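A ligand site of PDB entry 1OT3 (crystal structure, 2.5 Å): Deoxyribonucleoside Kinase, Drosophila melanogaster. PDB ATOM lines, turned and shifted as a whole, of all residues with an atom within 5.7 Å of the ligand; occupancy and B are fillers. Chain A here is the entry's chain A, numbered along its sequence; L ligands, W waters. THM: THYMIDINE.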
ATOM      1  N   ILE A  29     -21.096  27.294 -16.771  1.00  0.00           N
ATOM      2  CA  ILE A  29     -21.569  27.652 -15.450  1.00  0.00           C
ATOM      3  C   ILE A  29     -20.369  28.251 -14.717  1.00  0.00           C
ATOM      4  O   ILE A  29     -19.270  27.691 -14.757  1.00  0.00           O
ATOM      5  CB  ILE A  29     -22.047  26.428 -14.721  1.00  0.00           C
ATOM      6  CG1 ILE A  29     -22.953  25.620 -15.663  1.00  0.00           C
ATOM      7  CG2 ILE A  29     -22.767  26.845 -13.450  1.00  0.00           C
ATOM      8  CD1 ILE A  29     -23.473  24.334 -15.039  1.00  0.00           C
ATOM      9  N   LYS A  33     -21.183  35.297 -16.108  1.00  0.00           N
ATOM     10  CA  LYS A  33     -22.251  35.892 -16.883  1.00  0.00           C
ATOM     11  C   LYS A  33     -23.201  36.806 -16.127  1.00  0.00           C
ATOM     12  O   LYS A  33     -23.646  37.812 -16.679  1.00  0.00           O
ATOM     13  CB  LYS A  33     -23.062  34.804 -17.580  1.00  0.00           C
ATOM     14  CG  LYS A  33     -22.389  34.260 -18.822  1.00  0.00           C
ATOM     15  CD  LYS A  33     -23.339  33.376 -19.619  1.00  0.00           C
ATOM     16  CE  LYS A  33     -23.358  31.928 -19.116  1.00  0.00           C
ATOM     17  NZ  LYS A  33     -23.819  31.765 -17.704  1.00  0.00           N
ATOM     18  N   GLU A  52     -31.259  35.365 -17.606  1.00  0.00           N
ATOM     19  CA  GLU A  52     -31.691  33.968 -17.599  1.00  0.00           C
ATOM     20  C   GLU A  52     -32.826  33.761 -16.557  1.00  0.00           C
ATOM     21  O   GLU A  52     -32.667  34.081 -15.376  1.00  0.00           O
ATOM     22  CB  GLU A  52     -30.465  33.103 -17.326  1.00  0.00           C
ATOM     23  CG  GLU A  52     -30.690  31.631 -17.345  1.00  0.00           C
ATOM     24  CD  GLU A  52     -29.390  30.868 -17.171  1.00  0.00           C
ATOM     25  OE1 GLU A  52     -28.657  31.123 -16.188  1.00  0.00           O
ATOM     26  OE2 GLU A  52     -29.106  30.018 -18.032  1.00  0.00           O
ATOM     27  N   VAL A  54     -33.922  32.103 -14.307  1.00  0.00           N
ATOM     28  CA  VAL A  54     -33.640  31.234 -13.197  1.00  0.00           C
ATOM     29  C   VAL A  54     -34.719  31.328 -12.118  1.00  0.00           C
ATOM     30  O   VAL A  54     -35.042  30.337 -11.463  1.00  0.00           O
ATOM     31  CB  VAL A  54     -32.299  31.570 -12.570  1.00  0.00           C
ATOM     32  CG1 VAL A  54     -31.973  30.550 -11.498  1.00  0.00           C
ATOM     33  CG2 VAL A  54     -31.211  31.575 -13.640  1.00  0.00           C
ATOM     34  N   TRP A  57     -37.421  29.008 -12.833  1.00  0.00           N
ATOM     35  CA  TRP A  57     -37.090  27.605 -12.631  1.00  0.00           C
ATOM     36  C   TRP A  57     -37.070  27.206 -11.143  1.00  0.00           C
ATOM     37  O   TRP A  57     -37.195  26.039 -10.786  1.00  0.00           O
ATOM     38  CB  TRP A  57     -35.743  27.254 -13.296  1.00  0.00           C
ATOM     39  CG  TRP A  57     -35.599  27.715 -14.729  1.00  0.00           C
ATOM     40  CD1 TRP A  57     -36.596  27.943 -15.626  1.00  0.00           C
ATOM     41  CD2 TRP A  57     -34.376  27.978 -15.419  1.00  0.00           C
ATOM     42  NE1 TRP A  57     -36.075  28.333 -16.824  1.00  0.00           N
ATOM     43  CE2 TRP A  57     -34.721  28.366 -16.731  1.00  0.00           C
ATOM     44  CE3 TRP A  57     -33.029  27.936 -15.050  1.00  0.00           C
ATOM     45  CZ2 TRP A  57     -33.755  28.707 -17.700  1.00  0.00           C
ATOM     46  CZ3 TRP A  57     -32.064  28.270 -15.998  1.00  0.00           C
ATOM     47  CH2 TRP A  57     -32.438  28.656 -17.320  1.00  0.00           C
ATOM     48  N   LEU A  66     -35.234  23.427 -10.722  1.00  0.00           N
ATOM     49  CA  LEU A  66     -33.772  23.492 -10.731  1.00  0.00           C
ATOM     50  C   LEU A  66     -33.195  22.675  -9.572  1.00  0.00           C
ATOM     51  O   LEU A  66     -32.255  21.911  -9.759  1.00  0.00           O
ATOM     52  CB  LEU A  66     -33.287  24.953 -10.646  1.00  0.00           C
ATOM     53  CG  LEU A  66     -31.773  25.207 -10.626  1.00  0.00           C
ATOM     54  CD1 LEU A  66     -31.163  24.715 -11.932  1.00  0.00           C
ATOM     55  CD2 LEU A  66     -31.493  26.702 -10.430  1.00  0.00           C
ATOM     56  N   MET A  69     -33.875  18.942 -10.125  1.00  0.00           N
ATOM     57  CA  MET A  69     -33.032  18.399 -11.190  1.00  0.00           C
ATOM     58  C   MET A  69     -31.648  18.062 -10.676  1.00  0.00           C
ATOM     59  O   MET A  69     -31.085  17.021 -11.022  1.00  0.00           O
ATOM     60  CB  MET A  69     -32.897  19.402 -12.351  1.00  0.00           C
ATOM     61  CG  MET A  69     -32.095  18.902 -13.549  1.00  0.00           C
ATOM     62  SD  MET A  69     -30.305  18.977 -13.307  1.00  0.00           S
ATOM     63  CE  MET A  69     -30.045  20.767 -13.218  1.00  0.00           C
ATOM     64  N   TYR A  70     -31.094  18.952  -9.853  1.00  0.00           N
ATOM     65  CA  TYR A  70     -29.761  18.733  -9.316  1.00  0.00           C
ATOM     66  C   TYR A  70     -29.707  17.639  -8.247  1.00  0.00           C
ATOM     67  O   TYR A  70     -28.682  16.980  -8.103  1.00  0.00           O
ATOM     68  CB  TYR A  70     -29.175  20.055  -8.800  1.00  0.00           C
ATOM     69  CG  TYR A  70     -28.396  20.831  -9.852  1.00  0.00           C
ATOM     70  CD1 TYR A  70     -28.801  22.108 -10.241  1.00  0.00           C
ATOM     71  CD2 TYR A  70     -27.258  20.288 -10.449  1.00  0.00           C
ATOM     72  CE1 TYR A  70     -28.082  22.838 -11.187  1.00  0.00           C
ATOM     73  CE2 TYR A  70     -26.532  20.998 -11.401  1.00  0.00           C
ATOM     74  CZ  TYR A  70     -26.954  22.285 -11.764  1.00  0.00           C
ATOM     75  OH  TYR A  70     -26.245  23.035 -12.689  1.00  0.00           O
ATOM     76  N   PHE A  80     -37.512  19.440 -16.180  1.00  0.00           N
ATOM     77  CA  PHE A  80     -36.783  20.678 -16.018  1.00  0.00           C
ATOM     78  C   PHE A  80     -36.324  21.304 -17.343  1.00  0.00           C
ATOM     79  O   PHE A  80     -36.544  22.512 -17.583  1.00  0.00           O
ATOM     80  CB  PHE A  80     -35.578  20.458 -15.111  1.00  0.00           C
ATOM     81  CG  PHE A  80     -34.602  21.585 -15.114  1.00  0.00           C
ATOM     82  CD1 PHE A  80     -34.945  22.830 -14.592  1.00  0.00           C
ATOM     83  CD2 PHE A  80     -33.337  21.406 -15.645  1.00  0.00           C
ATOM     84  CE1 PHE A  80     -34.038  23.882 -14.610  1.00  0.00           C
ATOM     85  CE2 PHE A  80     -32.425  22.444 -15.677  1.00  0.00           C
ATOM     86  CZ  PHE A  80     -32.780  23.692 -15.149  1.00  0.00           C
ATOM     87  N   GLN A  81     -35.694  20.492 -18.193  1.00  0.00           N
ATOM     88  CA  GLN A  81     -35.216  20.954 -19.495  1.00  0.00           C
ATOM     89  C   GLN A  81     -36.379  21.366 -20.396  1.00  0.00           C
ATOM     90  O   GLN A  81     -36.224  22.236 -21.256  1.00  0.00           O
ATOM     91  CB  GLN A  81     -34.388  19.869 -20.180  1.00  0.00           C
ATOM     92  CG  GLN A  81     -32.994  19.737 -19.600  1.00  0.00           C
ATOM     93  CD  GLN A  81     -32.231  21.040 -19.633  1.00  0.00           C
ATOM     94  OE1 GLN A  81     -31.207  21.177 -18.995  1.00  0.00           O
ATOM     95  NE2 GLN A  81     -32.745  22.001 -20.378  1.00  0.00           N
ATOM     96  N   VAL A  84     -37.210  24.711 -19.230  1.00  0.00           N
ATOM     97  CA  VAL A  84     -36.156  25.619 -19.658  1.00  0.00           C
ATOM     98  C   VAL A  84     -36.437  26.001 -21.127  1.00  0.00           C
ATOM     99  O   VAL A  84     -36.434  27.181 -21.476  1.00  0.00           O
ATOM    100  CB  VAL A  84     -34.775  24.945 -19.609  1.00  0.00           C
ATOM    101  CG1 VAL A  84     -33.726  25.790 -20.359  1.00  0.00           C
ATOM    102  CG2 VAL A  84     -34.385  24.748 -18.141  1.00  0.00           C
ATOM    103  N   MET A  88     -37.221  29.963 -22.280  1.00  0.00           N
ATOM    104  CA  MET A  88     -36.230  30.470 -23.209  1.00  0.00           C
ATOM    105  C   MET A  88     -36.945  30.888 -24.507  1.00  0.00           C
ATOM    106  O   MET A  88     -36.621  31.902 -25.141  1.00  0.00           O
ATOM    107  CB  MET A  88     -35.191  29.370 -23.479  1.00  0.00           C
ATOM    108  CG  MET A  88     -33.827  29.863 -23.760  1.00  0.00           C
ATOM    109  SD  MET A  88     -33.190  30.798 -22.415  1.00  0.00           S
ATOM    110  CE  MET A  88     -32.088  29.747 -21.559  1.00  0.00           C
ATOM    111  N   ARG A 105     -27.905  33.412 -22.147  1.00  0.00           N
ATOM    112  CA  ARG A 105     -28.166  32.028 -22.547  1.00  0.00           C
ATOM    113  C   ARG A 105     -29.306  32.006 -23.512  1.00  0.00           C
ATOM    114  O   ARG A 105     -29.975  33.017 -23.712  1.00  0.00           O
ATOM    115  CB  ARG A 105     -28.544  31.111 -21.371  1.00  0.00           C
ATOM    116  CG  ARG A 105     -27.388  30.862 -20.413  1.00  0.00           C
ATOM    117  CD  ARG A 105     -26.737  29.518 -20.672  1.00  0.00           C
ATOM    118  NE  ARG A 105     -25.579  29.297 -19.813  1.00  0.00           N
ATOM    119  CZ  ARG A 105     -25.635  28.948 -18.540  1.00  0.00           C
ATOM    120  NH1 ARG A 105     -26.801  28.775 -17.957  1.00  0.00           N
ATOM    121  NH2 ARG A 105     -24.536  28.859 -17.823  1.00  0.00           N
ATOM    122  N   SER A 106     -29.594  30.854 -24.063  1.00  0.00           N
ATOM    123  CA  SER A 106     -30.645  30.793 -25.053  1.00  0.00           C
ATOM    124  C   SER A 106     -31.190  29.414 -25.216  1.00  0.00           C
ATOM    125  O   SER A 106     -30.862  28.503 -24.471  1.00  0.00           O
ATOM    126  CB  SER A 106     -30.068  31.197 -26.401  1.00  0.00           C
ATOM    127  OG  SER A 106     -29.082  30.232 -26.783  1.00  0.00           O
ATOM    128  N   SER A 109     -28.069  27.126 -26.283  1.00  0.00           N
ATOM    129  CA  SER A 109     -27.230  26.607 -25.214  1.00  0.00           C
ATOM    130  C   SER A 109     -27.940  25.472 -24.468  1.00  0.00           C
ATOM    131  O   SER A 109     -27.298  24.542 -24.007  1.00  0.00           O
ATOM    132  CB  SER A 109     -26.824  27.737 -24.250  1.00  0.00           C
ATOM    133  OG  SER A 109     -27.910  28.621 -23.965  1.00  0.00           O
ATOM    134  N   ALA A 110     -29.264  25.553 -24.336  1.00  0.00           N
ATOM    135  CA  ALA A 110     -30.034  24.522 -23.647  1.00  0.00           C
ATOM    136  C   ALA A 110     -29.962  23.226 -24.428  1.00  0.00           C
ATOM    137  O   ALA A 110     -29.829  22.135 -23.856  1.00  0.00           O
ATOM    138  CB  ALA A 110     -31.517  24.960 -23.510  1.00  0.00           C
ATOM    139  N   PHE A 114     -26.423  21.809 -22.553  1.00  0.00           N
ATOM    140  CA  PHE A 114     -27.083  21.193 -21.429  1.00  0.00           C
ATOM    141  C   PHE A 114     -27.846  19.903 -21.702  1.00  0.00           C
ATOM    142  O   PHE A 114     -27.586  18.901 -21.029  1.00  0.00           O
ATOM    143  CB  PHE A 114     -27.944  22.238 -20.719  1.00  0.00           C
ATOM    144  CG  PHE A 114     -27.125  23.314 -20.050  1.00  0.00           C
ATOM    145  CD1 PHE A 114     -26.822  24.499 -20.714  1.00  0.00           C
ATOM    146  CD2 PHE A 114     -26.584  23.114 -18.778  1.00  0.00           C
ATOM    147  CE1 PHE A 114     -26.003  25.445 -20.137  1.00  0.00           C
ATOM    148  CE2 PHE A 114     -25.762  24.077 -18.187  1.00  0.00           C
ATOM    149  CZ  PHE A 114     -25.472  25.242 -18.867  1.00  0.00           C
ATOM    150  N   VAL A 115     -28.739  19.879 -22.688  1.00  0.00           N
ATOM    151  CA  VAL A 115     -29.480  18.641 -22.929  1.00  0.00           C
ATOM    152  C   VAL A 115     -28.561  17.553 -23.483  1.00  0.00           C
ATOM    153  O   VAL A 115     -28.644  16.395 -23.057  1.00  0.00           O
ATOM    154  CB  VAL A 115     -30.683  18.868 -23.871  1.00  0.00           C
ATOM    155  CG1 VAL A 115     -31.237  17.528 -24.341  1.00  0.00           C
ATOM    156  CG2 VAL A 115     -31.775  19.639 -23.125  1.00  0.00           C
ATOM    157  N   MET A 118     -26.679  15.886 -20.783  1.00  0.00           N
ATOM    158  CA  MET A 118     -27.520  15.076 -19.916  1.00  0.00           C
ATOM    159  C   MET A 118     -27.946  13.778 -20.605  1.00  0.00           C
ATOM    160  O   MET A 118     -28.473  12.869 -19.973  1.00  0.00           O
ATOM    161  CB  MET A 118     -28.756  15.850 -19.485  1.00  0.00           C
ATOM    162  CG  MET A 118     -28.547  16.766 -18.325  1.00  0.00           C
ATOM    163  SD  MET A 118     -29.929  17.912 -18.237  1.00  0.00           S
ATOM    164  CE  MET A 118     -29.139  19.311 -17.413  1.00  0.00           C
ATOM    165  N   GLU A 171     -27.779  25.467  -5.864  1.00  0.00           N
ATOM    166  CA  GLU A 171     -28.098  24.114  -6.306  1.00  0.00           C
ATOM    167  C   GLU A 171     -26.988  23.487  -7.156  1.00  0.00           C
ATOM    168  O   GLU A 171     -26.760  22.277  -7.072  1.00  0.00           O
ATOM    169  CB  GLU A 171     -29.395  24.122  -7.104  1.00  0.00           C
ATOM    170  CG  GLU A 171     -30.613  24.659  -6.345  1.00  0.00           C
ATOM    171  CD  GLU A 171     -30.863  26.147  -6.566  1.00  0.00           C
ATOM    172  OE1 GLU A 171     -29.893  26.918  -6.706  1.00  0.00           O
ATOM    173  OE2 GLU A 171     -32.038  26.539  -6.586  1.00  0.00           O
ATOM    174  N   GLU A 172     -26.302  24.324  -7.941  1.00  0.00           N
ATOM    175  CA  GLU A 172     -25.225  23.908  -8.837  1.00  0.00           C
ATOM    176  C   GLU A 172     -23.851  23.839  -8.166  1.00  0.00           C
ATOM    177  O   GLU A 172     -22.879  23.384  -8.775  1.00  0.00           O
ATOM    178  CB  GLU A 172     -25.116  24.894  -9.994  1.00  0.00           C
ATOM    179  CG  GLU A 172     -24.459  26.236  -9.598  1.00  0.00           C
ATOM    180  CD  GLU A 172     -24.978  27.432 -10.414  1.00  0.00           C
ATOM    181  OE1 GLU A 172     -24.164  28.269 -10.849  1.00  0.00           O
ATOM    182  OE2 GLU A 172     -26.217  27.530 -10.599  1.00  0.00           O
ATOM    183  N   TYR A 179     -18.114  17.667 -14.816  1.00  0.00           N
ATOM    184  CA  TYR A 179     -19.323  18.231 -15.387  1.00  0.00           C
ATOM    185  C   TYR A 179     -19.035  19.550 -16.116  1.00  0.00           C
ATOM    186  O   TYR A 179     -19.410  19.718 -17.269  1.00  0.00           O
ATOM    187  CB  TYR A 179     -20.341  18.450 -14.272  1.00  0.00           C
ATOM    188  CG  TYR A 179     -21.733  18.787 -14.716  1.00  0.00           C
ATOM    189  CD1 TYR A 179     -22.493  17.885 -15.470  1.00  0.00           C
ATOM    190  CD2 TYR A 179     -22.310  19.996 -14.349  1.00  0.00           C
ATOM    191  CE1 TYR A 179     -23.810  18.189 -15.834  1.00  0.00           C
ATOM    192  CE2 TYR A 179     -23.631  20.307 -14.707  1.00  0.00           C
ATOM    193  CZ  TYR A 179     -24.362  19.407 -15.436  1.00  0.00           C
ATOM    194  OH  TYR A 179     -25.664  19.711 -15.749  1.00  0.00           O
HETATM  195  O5' THM L   1     -27.376  29.117 -15.181  1.00  0.00           O
HETATM  196  C5' THM L   1     -28.584  28.738 -14.561  1.00  0.00           C
HETATM  197  C4' THM L   1     -28.474  27.339 -13.844  1.00  0.00           C
HETATM  198  O4' THM L   1     -29.175  26.247 -14.385  1.00  0.00           O
HETATM  199  C3' THM L   1     -27.110  26.578 -13.597  1.00  0.00           C
HETATM  200  O3' THM L   1     -26.985  25.698 -12.384  1.00  0.00           O
HETATM  201  C2' THM L   1     -27.013  26.013 -15.012  1.00  0.00           C
HETATM  202  C1' THM L   1     -28.352  25.352 -15.113  1.00  0.00           C
HETATM  203  N1  THM L   1     -28.962  25.177 -16.459  1.00  0.00           N
HETATM  204  C2  THM L   1     -29.321  23.925 -16.855  1.00  0.00           C
HETATM  205  O2  THM L   1     -29.133  22.964 -16.034  1.00  0.00           O
HETATM  206  N3  THM L   1     -29.861  23.674 -18.051  1.00  0.00           N
HETATM  207  C4  THM L   1     -30.052  24.663 -18.915  1.00  0.00           C
HETATM  208  O4  THM L   1     -30.580  24.394 -20.074  1.00  0.00           O
HETATM  209  C5  THM L   1     -29.689  25.982 -18.568  1.00  0.00           C
HETATM  210  C5M THM L   1     -29.910  27.135 -19.548  1.00  0.00           C
HETATM  211  C6  THM L   1     -29.127  26.235 -17.291  1.00  0.00           C
HETATM  212  O   HOH W   1     -24.639  29.591 -15.105  1.00  0.00           O
HETATM  213  O   HOH W   2     -26.844  22.119 -15.226  1.00  0.00           O
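The side-chain carboxylate (OE2) of Glu 52 is in salt-bridge range of the guanidinium group (NH1) of Arg 105, 2.6 Å away. The side-chain sulfur (SD) of Met 118 sits close to the side-chain amide oxygen (OE1) of Gln 81, at 3.6 Å. The backbone carbonyl oxygen of Ser 109 sits at hydrogen-bond distance from the backbone NH of Phe 114, at 3.2 Å. The backbone NH (N) of Leu 66 sits at hydrogen-bond distance from the backbone carbonyl oxygen (O) of Trp 57, at 3.3 Å. The backbone NH (N) of Val 115 sits at hydrogen-bond distance from the backbone carbonyl oxygen (O) of Ala 110 (2.8 Å).
CD1 of Ile 29 touches C2' of the ligand, at 3.9 Å. Val 54 touches the ligand (CG2 to C5', 3.97 Å). CH2 of Trp 57 touches C5M of the ligand (3.7 Å). Leu 66 touches the ligand (CD1 to O4', 3.5 Å). Met 69 touches the ligand (CE to O2, 3.7 Å). Phe 80 touches the ligand (CE2 to O2, 3.4 Å). CG1 of Val 84 touches O4 of the ligand, at 3.5 Å. Met 88 touches the ligand (CE to C5M, 3.95 Å). Ala 110 touches the ligand (CB to O4, 3.6 Å). Phe 114 touches the ligand. CE of Met 118 touches O2 of the ligand, 3.9 Å away. Hydrophobic or aromatic side chains that line the ligand: Ile 29, Val 54, Trp 57, Leu 66, Met 69, Tyr 70, Phe 80, Val 84, Met 88, Ala 110, Phe 114 and Met 118.
The side-chain carboxylate (OE1) of Glu 52 lies within hydrogen-bond range of an oxygen (O5') of the ligand, 2.6 Å away. The side-chain carboxylate (OE2) of Glu 172 lies within hydrogen-bond range of an oxygen (O3') of the ligand (2.7 Å). O3' of the ligand sits at hydrogen-bond distance from OH of Tyr 70. O5' of the ligand sits at hydrogen-bond distance from NH1 of Arg 105. OE1 of Gln 81 is in hydrogen-bond range of N3 of the ligand, 3.0 Å away.
Water W2 lies within hydrogen-bond range of an oxygen (O2) of the ligand (2.6 Å), the side-chain hydroxyl of Tyr 179 (2.7 Å) and the side-chain hydroxyl of Tyr 70 (2.8 Å). Water W1 lies within hydrogen-bond range of O5' of the ligand (2.8 Å), NH2 of Arg 105 (2.8 Å) and NZ of Lys 33 (3.5 Å).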
